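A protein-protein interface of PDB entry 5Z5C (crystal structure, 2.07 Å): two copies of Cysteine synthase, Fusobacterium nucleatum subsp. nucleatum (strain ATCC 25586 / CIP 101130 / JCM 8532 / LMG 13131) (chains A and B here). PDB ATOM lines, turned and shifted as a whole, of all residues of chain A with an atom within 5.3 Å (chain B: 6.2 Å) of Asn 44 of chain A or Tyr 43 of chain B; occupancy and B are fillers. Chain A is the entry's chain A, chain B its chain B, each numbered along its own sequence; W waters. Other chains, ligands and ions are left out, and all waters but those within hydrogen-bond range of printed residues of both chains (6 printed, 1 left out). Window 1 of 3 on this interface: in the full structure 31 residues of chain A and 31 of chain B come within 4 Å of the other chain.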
ATOM      1  N   ASN A  15       5.451 -14.788 -25.106  1.00  0.00           N
ATOM      2  CA  ASN A  15       5.555 -16.112 -24.468  1.00  0.00           C
ATOM      3  C   ASN A  15       4.228 -16.586 -23.914  1.00  0.00           C
ATOM      4  O   ASN A  15       4.146 -17.693 -23.459  1.00  0.00           O
ATOM      5  CB  ASN A  15       6.615 -16.072 -23.367  1.00  0.00           C
ATOM      6  CG  ASN A  15       8.007 -15.866 -23.934  1.00  0.00           C
ATOM      7  OD1 ASN A  15       8.325 -16.469 -24.919  1.00  0.00           O
ATOM      8  ND2 ASN A  15       8.806 -14.977 -23.344  1.00  0.00           N
ATOM      9  N   LEU A  16       3.190 -15.742 -23.923  1.00  0.00           N
ATOM     10  CA  LEU A  16       1.853 -16.126 -23.488  1.00  0.00           C
ATOM     11  C   LEU A  16       1.027 -16.767 -24.590  1.00  0.00           C
ATOM     12  O   LEU A  16      -0.073 -17.222 -24.307  1.00  0.00           O
ATOM     13  CB  LEU A  16       1.078 -14.924 -22.907  1.00  0.00           C
ATOM     14  CG  LEU A  16       1.665 -14.297 -21.672  1.00  0.00           C
ATOM     15  CD1 LEU A  16       0.952 -13.004 -21.318  1.00  0.00           C
ATOM     16  CD2 LEU A  16       1.602 -15.283 -20.498  1.00  0.00           C
ATOM     17  N   VAL A  17       1.516 -16.778 -25.825  1.00  0.00           N
ATOM     18  CA  VAL A  17       0.719 -17.285 -26.964  1.00  0.00           C
ATOM     19  C   VAL A  17       1.565 -18.159 -27.847  1.00  0.00           C
ATOM     20  O   VAL A  17       2.757 -18.085 -27.835  1.00  0.00           O
ATOM     21  CB  VAL A  17       0.071 -16.173 -27.820  1.00  0.00           C
ATOM     22  CG1 VAL A  17      -0.783 -15.233 -26.934  1.00  0.00           C
ATOM     23  CG2 VAL A  17       1.132 -15.376 -28.606  1.00  0.00           C
ATOM     24  N   GLY A  18       0.930 -19.001 -28.641  1.00  0.00           N
ATOM     25  CA  GLY A  18       1.666 -19.738 -29.604  1.00  0.00           C
ATOM     26  C   GLY A  18       2.429 -20.924 -29.043  1.00  0.00           C
ATOM     27  O   GLY A  18       2.336 -21.257 -27.846  1.00  0.00           O
ATOM     28  N   THR A  20       2.018 -24.117 -29.879  1.00  0.00           N
ATOM     29  CA  THR A  20       1.013 -25.047 -29.431  1.00  0.00           C
ATOM     30  C   THR A  20       1.322 -26.462 -30.013  1.00  0.00           C
ATOM     31  O   THR A  20       2.132 -26.576 -30.949  1.00  0.00           O
ATOM     32  CB  THR A  20      -0.361 -24.602 -29.918  1.00  0.00           C
ATOM     33  OG1 THR A  20      -0.387 -24.598 -31.359  1.00  0.00           O
ATOM     34  CG2 THR A  20      -0.725 -23.185 -29.383  1.00  0.00           C
ATOM     35  N   GLU A  41      -5.170 -25.222 -30.433  1.00  0.00           N
ATOM     36  CA  GLU A  41      -4.982 -23.822 -30.058  1.00  0.00           C
ATOM     37  C   GLU A  41      -5.603 -23.405 -28.753  1.00  0.00           C
ATOM     38  O   GLU A  41      -5.585 -22.223 -28.369  1.00  0.00           O
ATOM     39  CB  GLU A  41      -5.408 -22.933 -31.236  1.00  0.00           C
ATOM     40  CG  GLU A  41      -4.538 -23.107 -32.462  1.00  0.00           C
ATOM     41  CD  GLU A  41      -3.130 -22.605 -32.215  1.00  0.00           C
ATOM     42  OE1 GLU A  41      -2.991 -21.522 -31.624  1.00  0.00           O
ATOM     43  OE2 GLU A  41      -2.155 -23.283 -32.613  1.00  0.00           O
ATOM     44  N   SER A  42      -6.068 -24.383 -27.994  1.00  0.00           N
ATOM     45  CA  SER A  42      -6.466 -24.136 -26.626  1.00  0.00           C
ATOM     46  C   SER A  42      -5.276 -23.727 -25.703  1.00  0.00           C
ATOM     47  O   SER A  42      -5.503 -23.158 -24.630  1.00  0.00           O
ATOM     48  CB  SER A  42      -7.172 -25.376 -26.055  1.00  0.00           C
ATOM     49  OG  SER A  42      -6.196 -26.374 -25.802  1.00  0.00           O
ATOM     50  N   TYR A  43      -4.034 -24.032 -26.114  1.00  0.00           N
ATOM     51  CA  TYR A  43      -2.863 -23.862 -25.273  1.00  0.00           C
ATOM     52  C   TYR A  43      -2.357 -22.410 -25.440  1.00  0.00           C
ATOM     53  O   TYR A  43      -1.279 -22.165 -25.943  1.00  0.00           O
ATOM     54  CB  TYR A  43      -1.731 -24.760 -25.723  1.00  0.00           C
ATOM     55  CG  TYR A  43      -1.912 -26.268 -25.379  1.00  0.00           C
ATOM     56  CD1 TYR A  43      -2.872 -27.041 -26.018  1.00  0.00           C
ATOM     57  CD2 TYR A  43      -1.091 -26.886 -24.444  1.00  0.00           C
ATOM     58  CE1 TYR A  43      -3.028 -28.424 -25.718  1.00  0.00           C
ATOM     59  CE2 TYR A  43      -1.234 -28.252 -24.140  1.00  0.00           C
ATOM     60  CZ  TYR A  43      -2.201 -29.005 -24.781  1.00  0.00           C
ATOM     61  OH  TYR A  43      -2.326 -30.339 -24.474  1.00  0.00           O
ATOM     62  N   ASN A  44      -3.179 -21.449 -25.016  1.00  0.00           N
ATOM     63  CA  ASN A  44      -2.971 -20.029 -25.312  1.00  0.00           C
ATOM     64  C   ASN A  44      -3.604 -19.284 -24.149  1.00  0.00           C
ATOM     65  O   ASN A  44      -4.510 -19.846 -23.498  1.00  0.00           O
ATOM     66  CB  ASN A  44      -3.716 -19.637 -26.576  1.00  0.00           C
ATOM     67  CG  ASN A  44      -2.884 -19.790 -27.826  1.00  0.00           C
ATOM     68  OD1 ASN A  44      -1.839 -19.157 -27.911  1.00  0.00           O
ATOM     69  ND2 ASN A  44      -3.379 -20.594 -28.837  1.00  0.00           N
ATOM     70  N   LEU A  45      -3.125 -18.045 -23.929  1.00  0.00           N
ATOM     71  CA  LEU A  45      -3.560 -17.173 -22.821  1.00  0.00           C
ATOM     72  C   LEU A  45      -5.018 -17.330 -22.428  1.00  0.00           C
ATOM     73  O   LEU A  45      -5.284 -17.521 -21.272  1.00  0.00           O
ATOM     74  CB  LEU A  45      -3.227 -15.677 -23.122  1.00  0.00           C
ATOM     75  CG  LEU A  45      -3.489 -14.644 -21.995  1.00  0.00           C
ATOM     76  CD1 LEU A  45      -2.563 -14.891 -20.818  1.00  0.00           C
ATOM     77  CD2 LEU A  45      -3.282 -13.231 -22.493  1.00  0.00           C
ATOM     78  N   THR A  46      -5.950 -17.151 -23.358  1.00  0.00           N
ATOM     79  CA  THR A  46      -7.358 -17.215 -23.091  1.00  0.00           C
ATOM     80  C   THR A  46      -8.023 -18.468 -23.708  1.00  0.00           C
ATOM     81  O   THR A  46      -9.234 -18.549 -23.678  1.00  0.00           O
ATOM     82  CB  THR A  46      -8.134 -15.925 -23.511  1.00  0.00           C
ATOM     83  OG1 THR A  46      -8.217 -15.784 -24.943  1.00  0.00           O
ATOM     84  CG2 THR A  46      -7.487 -14.650 -22.926  1.00  0.00           C
ATOM     85  N   GLY A  47      -7.226 -19.441 -24.192  1.00  0.00           N
ATOM     86  CA  GLY A  47      -7.715 -20.703 -24.736  1.00  0.00           C
ATOM     87  C   GLY A  47      -8.129 -20.738 -26.187  1.00  0.00           C
ATOM     88  O   GLY A  47      -8.899 -21.628 -26.594  1.00  0.00           O
ATOM     89  N   SER A  48      -7.610 -19.837 -27.012  1.00  0.00           N
ATOM     90  CA  SER A  48      -7.997 -19.809 -28.427  1.00  0.00           C
ATOM     91  C   SER A  48      -6.916 -19.269 -29.293  1.00  0.00           C
ATOM     92  O   SER A  48      -6.019 -18.514 -28.843  1.00  0.00           O
ATOM     93  CB  SER A  48      -9.278 -19.007 -28.662  1.00  0.00           C
ATOM     94  OG  SER A  48      -9.028 -17.669 -29.055  1.00  0.00           O
ATOM     95  N   ILE A  49      -7.029 -19.635 -30.557  1.00  0.00           N
ATOM     96  CA  ILE A  49      -6.194 -19.135 -31.634  1.00  0.00           C
ATOM     97  C   ILE A  49      -6.155 -17.607 -31.698  1.00  0.00           C
ATOM     98  O   ILE A  49      -5.151 -17.032 -32.140  1.00  0.00           O
ATOM     99  CB  ILE A  49      -6.626 -19.775 -32.983  1.00  0.00           C
ATOM    100  CG1 ILE A  49      -5.486 -19.710 -33.999  1.00  0.00           C
ATOM    101  CG2 ILE A  49      -7.957 -19.172 -33.460  1.00  0.00           C
ATOM    102  CD1 ILE A  49      -5.816 -20.380 -35.322  1.00  0.00           C
ATOM    103  N   ASP A  51      -5.825 -15.403 -29.507  1.00  0.00           N
ATOM    104  CA  ASP A  51      -4.782 -14.833 -28.674  1.00  0.00           C
ATOM    105  C   ASP A  51      -3.543 -14.430 -29.458  1.00  0.00           C
ATOM    106  O   ASP A  51      -2.915 -13.392 -29.196  1.00  0.00           O
ATOM    107  CB  ASP A  51      -4.382 -15.844 -27.599  1.00  0.00           C
ATOM    108  CG  ASP A  51      -5.442 -16.023 -26.527  1.00  0.00           C
ATOM    109  OD1 ASP A  51      -6.150 -14.996 -26.153  1.00  0.00           O
ATOM    110  OD2 ASP A  51      -5.573 -17.163 -26.019  1.00  0.00           O
ATOM    111  N   ARG A  52      -3.197 -15.277 -30.429  1.00  0.00           N
ATOM    112  CA  ARG A  52      -2.066 -15.015 -31.301  1.00  0.00           C
ATOM    113  C   ARG A  52      -2.295 -13.691 -32.042  1.00  0.00           C
ATOM    114  O   ARG A  52      -1.415 -12.873 -32.160  1.00  0.00           O
ATOM    115  CB  ARG A  52      -1.920 -16.137 -32.324  1.00  0.00           C
ATOM    116  CG  ARG A  52      -1.529 -17.488 -31.732  1.00  0.00           C
ATOM    117  CD  ARG A  52      -1.652 -18.582 -32.824  1.00  0.00           C
ATOM    118  NE  ARG A  52      -1.173 -19.909 -32.438  1.00  0.00           N
ATOM    119  CZ  ARG A  52       0.075 -20.349 -32.630  1.00  0.00           C
ATOM    120  NH1 ARG A  52       1.037 -19.503 -32.996  1.00  0.00           N
ATOM    121  NH2 ARG A  52       0.369 -21.628 -32.406  1.00  0.00           N
ATOM    122  N   ARG A 338       5.909 -30.323 -30.911  1.00  0.00           N
ATOM    123  CA  ARG A 338       5.866 -28.980 -30.317  1.00  0.00           C
ATOM    124  C   ARG A 338       7.268 -28.430 -30.197  1.00  0.00           C
ATOM    125  O   ARG A 338       8.093 -29.080 -29.560  1.00  0.00           O
ATOM    126  CB  ARG A 338       5.262 -29.070 -28.919  1.00  0.00           C
ATOM    127  CG  ARG A 338       4.520 -27.832 -28.477  1.00  0.00           C
ATOM    128  CD  ARG A 338       3.666 -28.167 -27.304  1.00  0.00           C
ATOM    129  NE  ARG A 338       3.183 -26.994 -26.605  1.00  0.00           N
ATOM    130  CZ  ARG A 338       2.716 -27.013 -25.369  1.00  0.00           C
ATOM    131  NH1 ARG A 338       2.618 -28.168 -24.712  1.00  0.00           N
ATOM    132  NH2 ARG A 338       2.314 -25.887 -24.796  1.00  0.00           N
ATOM    133  N   LEU B  16       1.847 -32.931 -24.656  1.00  0.00           N
ATOM    134  CA  LEU B  16       0.535 -32.404 -24.328  1.00  0.00           C
ATOM    135  C   LEU B  16       0.424 -31.712 -22.963  1.00  0.00           C
ATOM    136  O   LEU B  16      -0.650 -31.174 -22.662  1.00  0.00           O
ATOM    137  CB  LEU B  16      -0.513 -33.499 -24.448  1.00  0.00           C
ATOM    138  CG  LEU B  16      -0.651 -34.117 -25.851  1.00  0.00           C
ATOM    139  CD1 LEU B  16      -1.616 -35.280 -25.819  1.00  0.00           C
ATOM    140  CD2 LEU B  16      -1.127 -33.054 -26.857  1.00  0.00           C
ATOM    141  N   VAL B  17       1.497 -31.774 -22.156  1.00  0.00           N
ATOM    142  CA  VAL B  17       1.490 -31.301 -20.778  1.00  0.00           C
ATOM    143  C   VAL B  17       2.773 -30.599 -20.448  1.00  0.00           C
ATOM    144  O   VAL B  17       3.766 -30.793 -21.097  1.00  0.00           O
ATOM    145  CB  VAL B  17       1.260 -32.420 -19.737  1.00  0.00           C
ATOM    146  CG1 VAL B  17      -0.076 -33.103 -19.956  1.00  0.00           C
ATOM    147  CG2 VAL B  17       2.407 -33.463 -19.741  1.00  0.00           C
ATOM    148  N   GLY B  18       2.711 -29.720 -19.439  1.00  0.00           N
ATOM    149  CA  GLY B  18       3.843 -28.936 -18.987  1.00  0.00           C
ATOM    150  C   GLY B  18       4.355 -27.873 -19.919  1.00  0.00           C
ATOM    151  O   GLY B  18       3.641 -27.463 -20.858  1.00  0.00           O
ATOM    152  N   MLY B  19       5.572 -27.386 -19.596  1.00  0.00           N
ATOM    153  CA  MLY B  19       6.296 -26.293 -20.277  1.00  0.00           C
ATOM    154  CB  MLY B  19       6.723 -26.723 -21.685  1.00  0.00           C
ATOM    155  CG  MLY B  19       7.458 -28.067 -21.671  1.00  0.00           C
ATOM    156  CD  MLY B  19       7.516 -28.670 -23.079  1.00  0.00           C
ATOM    157  CE  MLY B  19       6.693 -29.953 -23.209  1.00  0.00           C
ATOM    158  NZ  MLY B  19       5.269 -29.651 -23.447  1.00  0.00           N
ATOM    159  C   MLY B  19       5.417 -25.080 -20.350  1.00  0.00           C
ATOM    160  O   MLY B  19       5.272 -24.467 -21.406  1.00  0.00           O
ATOM    161  N   THR B  20       4.835 -24.740 -19.205  1.00  0.00           N
ATOM    162  CA  THR B  20       3.916 -23.615 -19.054  1.00  0.00           C
ATOM    163  C   THR B  20       4.625 -22.322 -18.755  1.00  0.00           C
ATOM    164  O   THR B  20       5.745 -22.300 -18.288  1.00  0.00           O
ATOM    165  CB  THR B  20       2.900 -23.868 -17.924  1.00  0.00           C
ATOM    166  OG1 THR B  20       3.591 -24.061 -16.692  1.00  0.00           O
ATOM    167  CG2 THR B  20       2.058 -25.073 -18.223  1.00  0.00           C
ATOM    168  N   PRO B  21       3.987 -21.202 -19.044  1.00  0.00           N
ATOM    169  CA  PRO B  21       4.622 -19.898 -18.719  1.00  0.00           C
ATOM    170  C   PRO B  21       4.895 -19.665 -17.225  1.00  0.00           C
ATOM    171  O   PRO B  21       4.059 -20.037 -16.387  1.00  0.00           O
ATOM    172  CB  PRO B  21       3.596 -18.863 -19.191  1.00  0.00           C
ATOM    173  CG  PRO B  21       2.602 -19.590 -19.980  1.00  0.00           C
ATOM    174  CD  PRO B  21       2.653 -21.044 -19.610  1.00  0.00           C
ATOM    175  N   ASN B  40       1.550 -20.502 -14.757  1.00  0.00           N
ATOM    176  CA  ASN B  40       0.196 -20.612 -15.309  1.00  0.00           C
ATOM    177  C   ASN B  40      -0.112 -21.991 -15.933  1.00  0.00           C
ATOM    178  O   ASN B  40       0.170 -22.223 -17.113  1.00  0.00           O
ATOM    179  CB  ASN B  40      -0.004 -19.497 -16.342  1.00  0.00           C
ATOM    180  CG  ASN B  40      -1.467 -19.290 -16.678  1.00  0.00           C
ATOM    181  OD1 ASN B  40      -2.275 -20.222 -16.582  1.00  0.00           O
ATOM    182  ND2 ASN B  40      -1.804 -18.086 -17.145  1.00  0.00           N
ATOM    183  N   GLU B  41      -0.818 -22.822 -15.158  1.00  0.00           N
ATOM    184  CA  GLU B  41      -1.088 -24.224 -15.493  1.00  0.00           C
ATOM    185  C   GLU B  41      -2.380 -24.481 -16.290  1.00  0.00           C
ATOM    186  O   GLU B  41      -2.690 -25.614 -16.563  1.00  0.00           O
ATOM    187  CB  GLU B  41      -1.058 -25.030 -14.195  1.00  0.00           C
ATOM    188  CG  GLU B  41       0.332 -24.972 -13.569  1.00  0.00           C
ATOM    189  CD  GLU B  41       1.361 -25.656 -14.451  1.00  0.00           C
ATOM    190  OE1 GLU B  41       1.045 -26.725 -15.015  1.00  0.00           O
ATOM    191  OE2 GLU B  41       2.468 -25.105 -14.609  1.00  0.00           O
ATOM    192  N   SER B  42      -3.077 -23.401 -16.718  1.00  0.00           N
ATOM    193  CA  SER B  42      -4.122 -23.488 -17.748  1.00  0.00           C
ATOM    194  C   SER B  42      -3.598 -23.996 -19.137  1.00  0.00           C
ATOM    195  O   SER B  42      -4.351 -24.592 -19.921  1.00  0.00           O
ATOM    196  CB  SER B  42      -4.880 -22.156 -17.915  1.00  0.00           C
ATOM    197  OG  SER B  42      -4.105 -21.281 -18.713  1.00  0.00           O
ATOM    198  N   TYR B  43      -2.309 -23.810 -19.406  1.00  0.00           N
ATOM    199  CA  TYR B  43      -1.687 -24.176 -20.680  1.00  0.00           C
ATOM    200  C   TYR B  43      -1.344 -25.715 -20.714  1.00  0.00           C
ATOM    201  O   TYR B  43      -0.174 -26.117 -20.839  1.00  0.00           O
ATOM    202  CB  TYR B  43      -0.371 -23.425 -20.857  1.00  0.00           C
ATOM    203  CG  TYR B  43      -0.514 -21.917 -21.127  1.00  0.00           C
ATOM    204  CD1 TYR B  43      -0.840 -21.032 -20.106  1.00  0.00           C
ATOM    205  CD2 TYR B  43      -0.267 -21.392 -22.390  1.00  0.00           C
ATOM    206  CE1 TYR B  43      -0.948 -19.673 -20.348  1.00  0.00           C
ATOM    207  CE2 TYR B  43      -0.370 -20.031 -22.636  1.00  0.00           C
ATOM    208  CZ  TYR B  43      -0.713 -19.170 -21.611  1.00  0.00           C
ATOM    209  OH  TYR B  43      -0.807 -17.810 -21.853  1.00  0.00           O
ATOM    210  N   ASN B  44      -2.361 -26.549 -20.626  1.00  0.00           N
ATOM    211  CA  ASN B  44      -2.264 -27.973 -20.453  1.00  0.00           C
ATOM    212  C   ASN B  44      -3.421 -28.586 -21.183  1.00  0.00           C
ATOM    213  O   ASN B  44      -4.387 -27.897 -21.471  1.00  0.00           O
ATOM    214  CB  ASN B  44      -2.329 -28.338 -18.959  1.00  0.00           C
ATOM    215  CG  ASN B  44      -0.959 -28.383 -18.323  1.00  0.00           C
ATOM    216  OD1 ASN B  44      -0.122 -29.195 -18.742  1.00  0.00           O
ATOM    217  ND2 ASN B  44      -0.717 -27.540 -17.299  1.00  0.00           N
ATOM    218  N   LEU B  45      -3.362 -29.892 -21.432  1.00  0.00           N
ATOM    219  CA  LEU B  45      -4.392 -30.602 -22.214  1.00  0.00           C
ATOM    220  C   LEU B  45      -5.824 -30.260 -21.884  1.00  0.00           C
ATOM    221  O   LEU B  45      -6.573 -29.998 -22.767  1.00  0.00           O
ATOM    222  CB  LEU B  45      -4.223 -32.141 -22.088  1.00  0.00           C
ATOM    223  CG  LEU B  45      -5.173 -33.014 -22.890  1.00  0.00           C
ATOM    224  CD1 LEU B  45      -4.969 -32.811 -24.388  1.00  0.00           C
ATOM    225  CD2 LEU B  45      -4.975 -34.476 -22.522  1.00  0.00           C
ATOM    226  N   GLY B  47      -6.657 -28.038 -19.375  1.00  0.00           N
ATOM    227  CA  GLY B  47      -6.680 -26.719 -18.708  1.00  0.00           C
ATOM    228  C   GLY B  47      -6.193 -26.691 -17.263  1.00  0.00           C
ATOM    229  O   GLY B  47      -6.387 -25.667 -16.628  1.00  0.00           O
ATOM    230  N   SER B  48      -5.596 -27.783 -16.739  1.00  0.00           N
ATOM    231  CA  SER B  48      -5.154 -27.779 -15.335  1.00  0.00           C
ATOM    232  C   SER B  48      -3.811 -28.430 -15.076  1.00  0.00           C
ATOM    233  O   SER B  48      -3.381 -29.318 -15.800  1.00  0.00           O
ATOM    234  CB  SER B  48      -6.197 -28.433 -14.387  1.00  0.00           C
ATOM    235  OG  SER B  48      -6.011 -29.828 -14.194  1.00  0.00           O
ATOM    236  N   ARG B 338       9.205 -18.902 -20.928  1.00  0.00           N
ATOM    237  CA  ARG B 338       8.648 -20.131 -21.476  1.00  0.00           C
ATOM    238  C   ARG B 338       9.845 -20.929 -22.013  1.00  0.00           C
ATOM    239  O   ARG B 338      10.502 -20.492 -22.978  1.00  0.00           O
ATOM    240  CB  ARG B 338       7.682 -19.783 -22.615  1.00  0.00           C
ATOM    241  CG  ARG B 338       6.764 -20.934 -23.036  1.00  0.00           C
ATOM    242  CD  ARG B 338       5.473 -20.898 -22.251  1.00  0.00           C
ATOM    243  NE  ARG B 338       4.578 -22.002 -22.586  1.00  0.00           N
ATOM    244  CZ  ARG B 338       3.551 -21.919 -23.442  1.00  0.00           C
ATOM    245  NH1 ARG B 338       3.313 -20.784 -24.105  1.00  0.00           N
ATOM    246  NH2 ARG B 338       2.777 -22.971 -23.648  1.00  0.00           N
HETATM  247  O   HOH W   1      -6.004 -26.307 -22.913  1.00  0.00           O
HETATM  248  O   HOH W   2       0.881 -20.357 -25.746  1.00  0.00           O
HETATM  249  O   HOH W   3       1.375 -28.205 -21.840  1.00  0.00           O
HETATM  250  O   HOH W   4       1.257 -23.421 -26.196  1.00  0.00           O
HETATM  251  O   HOH W   5      -6.786 -23.765 -21.712  1.00  0.00           O
HETATM  252  O   HOH W   6      -5.076 -21.421 -21.315  1.00  0.00           O
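The guanidinium group (NH1) of Arg 338 of chain A sits at hydrogen-bond distance from NZ of MLY 19 of chain B (3.3 Å).
The guanidinium group of Arg 338 of chain A lies close to the guanidinium group of Arg 338 of chain B.
N of Leu 45 of chain A lies close to OH of Tyr 43 of chain B (3.1 Å).
O of Asn 15 of chain A sits at hydrogen-bond distance from NH1 of Arg 338 of chain B.
The side-chain hydroxyl (OH) of Tyr 43 of chain B is in hydrogen-bond range of the backbone carbonyl oxygen (O) of Leu 16 of chain A (2.6 Å).
The side-chain hydroxyl (OH) of Tyr 43 of chain A lies within hydrogen-bond range of the backbone carbonyl oxygen (O) of Leu 16 of chain B, at 2.6 Å.
OH of Tyr 43 of chain A lies close to N of Leu 45 of chain B (3.2 Å).
The side-chain amide nitrogen of Asn 44 of chain A sits at hydrogen-bond distance from the backbone carbonyl oxygen of Ser 48 of chain A (3.4 Å).
The backbone NH of Leu 45 of chain A sits at hydrogen-bond distance from the side-chain carboxylate of Asp 51 of chain A.
The side-chain amide nitrogen of Asn 44 of chain A is in hydrogen-bond range of the backbone carbonyl oxygen of Glu 41 of chain A, 2.8 Å away.
The backbone NH (N) of Gly 18 of chain B sits at hydrogen-bond distance from the side-chain amide oxygen (OD1) of Asn 44 of chain B (3.0 Å).
The backbone NH (N) of Gly 18 of chain A lies within hydrogen-bond range of the side-chain amide oxygen (OD1) of Asn 44 of chain A.
The backbone carbonyl oxygen (O) of Leu 16 of chain B is in hydrogen-bond range of the backbone NH (N) of Leu 45 of chain B (3.2 Å).
Among the printed residues, merely in contact across the chains: Asn 44 of chain A with Tyr 43 of chain B (3.6 Å), Tyr 43 of chain A with Asn 44 of chain B (3.7 Å), Tyr 43 of chain A with Tyr 43 of chain B (3.8 Å) and Gly 18 of chain A with Arg 338 of chain B (3.9 Å).
Of chain B, only Tyr 43 (3.6 Å) comes within 4 Å of Asn 44 of chain A.
Tyr 43 of chain B touches just these residues of chain A: Leu 16, Tyr 43, Asn 44 and Leu 45.
Printed residues of chain B within 4 Å of Gly 18 of chain A: Arg 338.
Of the printed residues of chain B, Tyr 43 of chain A touches Leu 16, Tyr 43, Asn 44 and Leu 45.
Printed residues of chain A within 4 Å of Arg 338 of chain B: Asn 15 (3.3 Å), Gly 18 (3.9 Å) and Arg 338 (3.2 Å).
Of the printed residues of chain A, Asn 44 of chain B touches Tyr 43 (3.7 Å).
The nearest residue of chain A that does not touch Tyr 43 of chain B is Arg 338 of chain A (4.7 Å).
Hydrophobic or aromatic side chains of chain A that line the printed part of chain B: Leu 16, Tyr 43 and Leu 45.
Of the 15 printed residues of chain B, 6 touch a printed residue of chain A.
Leu 16 of chain A touches Tyr 43 of chain B, and with the chains exchanged Tyr 43 of chain A touches Leu 16 of chain B.
Tyr 43 of chain B touches its own counterpart, Tyr 43 of chain A.
Tyr 43 of chain A touches Leu 45 of chain B, and with the chains exchanged Leu 45 of chain A touches Tyr 43 of chain B.
Arg 338 of chain B touches its own counterpart, Arg 338 of chain A.
12 positions are printed for both chains.
Of the 11 pairs that touch across the chains among the printed residues, 8 have their exchanged pair printed and touching as well.
Water W3 lies within hydrogen-bond range of O of Gly 18 of chain B (2.6 Å), O of Tyr 43 of chain B (2.8 Å) and NH1 of Arg 338 of chain A (3.1 Å).
Water W1 bridges O of Asn 44 of chain B (2.7 Å) and OG of Ser 42 of chain A (2.9 Å).
Water W2 lies within hydrogen-bond range of the backbone carbonyl oxygen (O) of Gly 18 of chain A (2.7 Å), the backbone carbonyl oxygen (O) of Tyr 43 of chain A (2.8 Å) and the guanidinium group (NH1) of Arg 338 of chain B (3.0 Å).
Water W6 bridges the backbone carbonyl oxygen of Asn 44 of chain A (2.8 Å) and the side-chain hydroxyl of Ser 42 of chain B (2.8 Å).
Water W4 lies within hydrogen-bond range of O of Tyr 43 of chain A (2.8 Å), O of Gly 18 of chain A (2.9 Å), NH2 of Arg 338 of chain B (3.0 Å) and NH2 of Arg 338 of chain A (3.0 Å).
Water W5 lies within hydrogen-bond range of the backbone carbonyl oxygen (O) of Ser 42 of chain B (3.1 Å) and the backbone carbonyl oxygen (O) of Ser 42 of chain A (3.2 Å).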
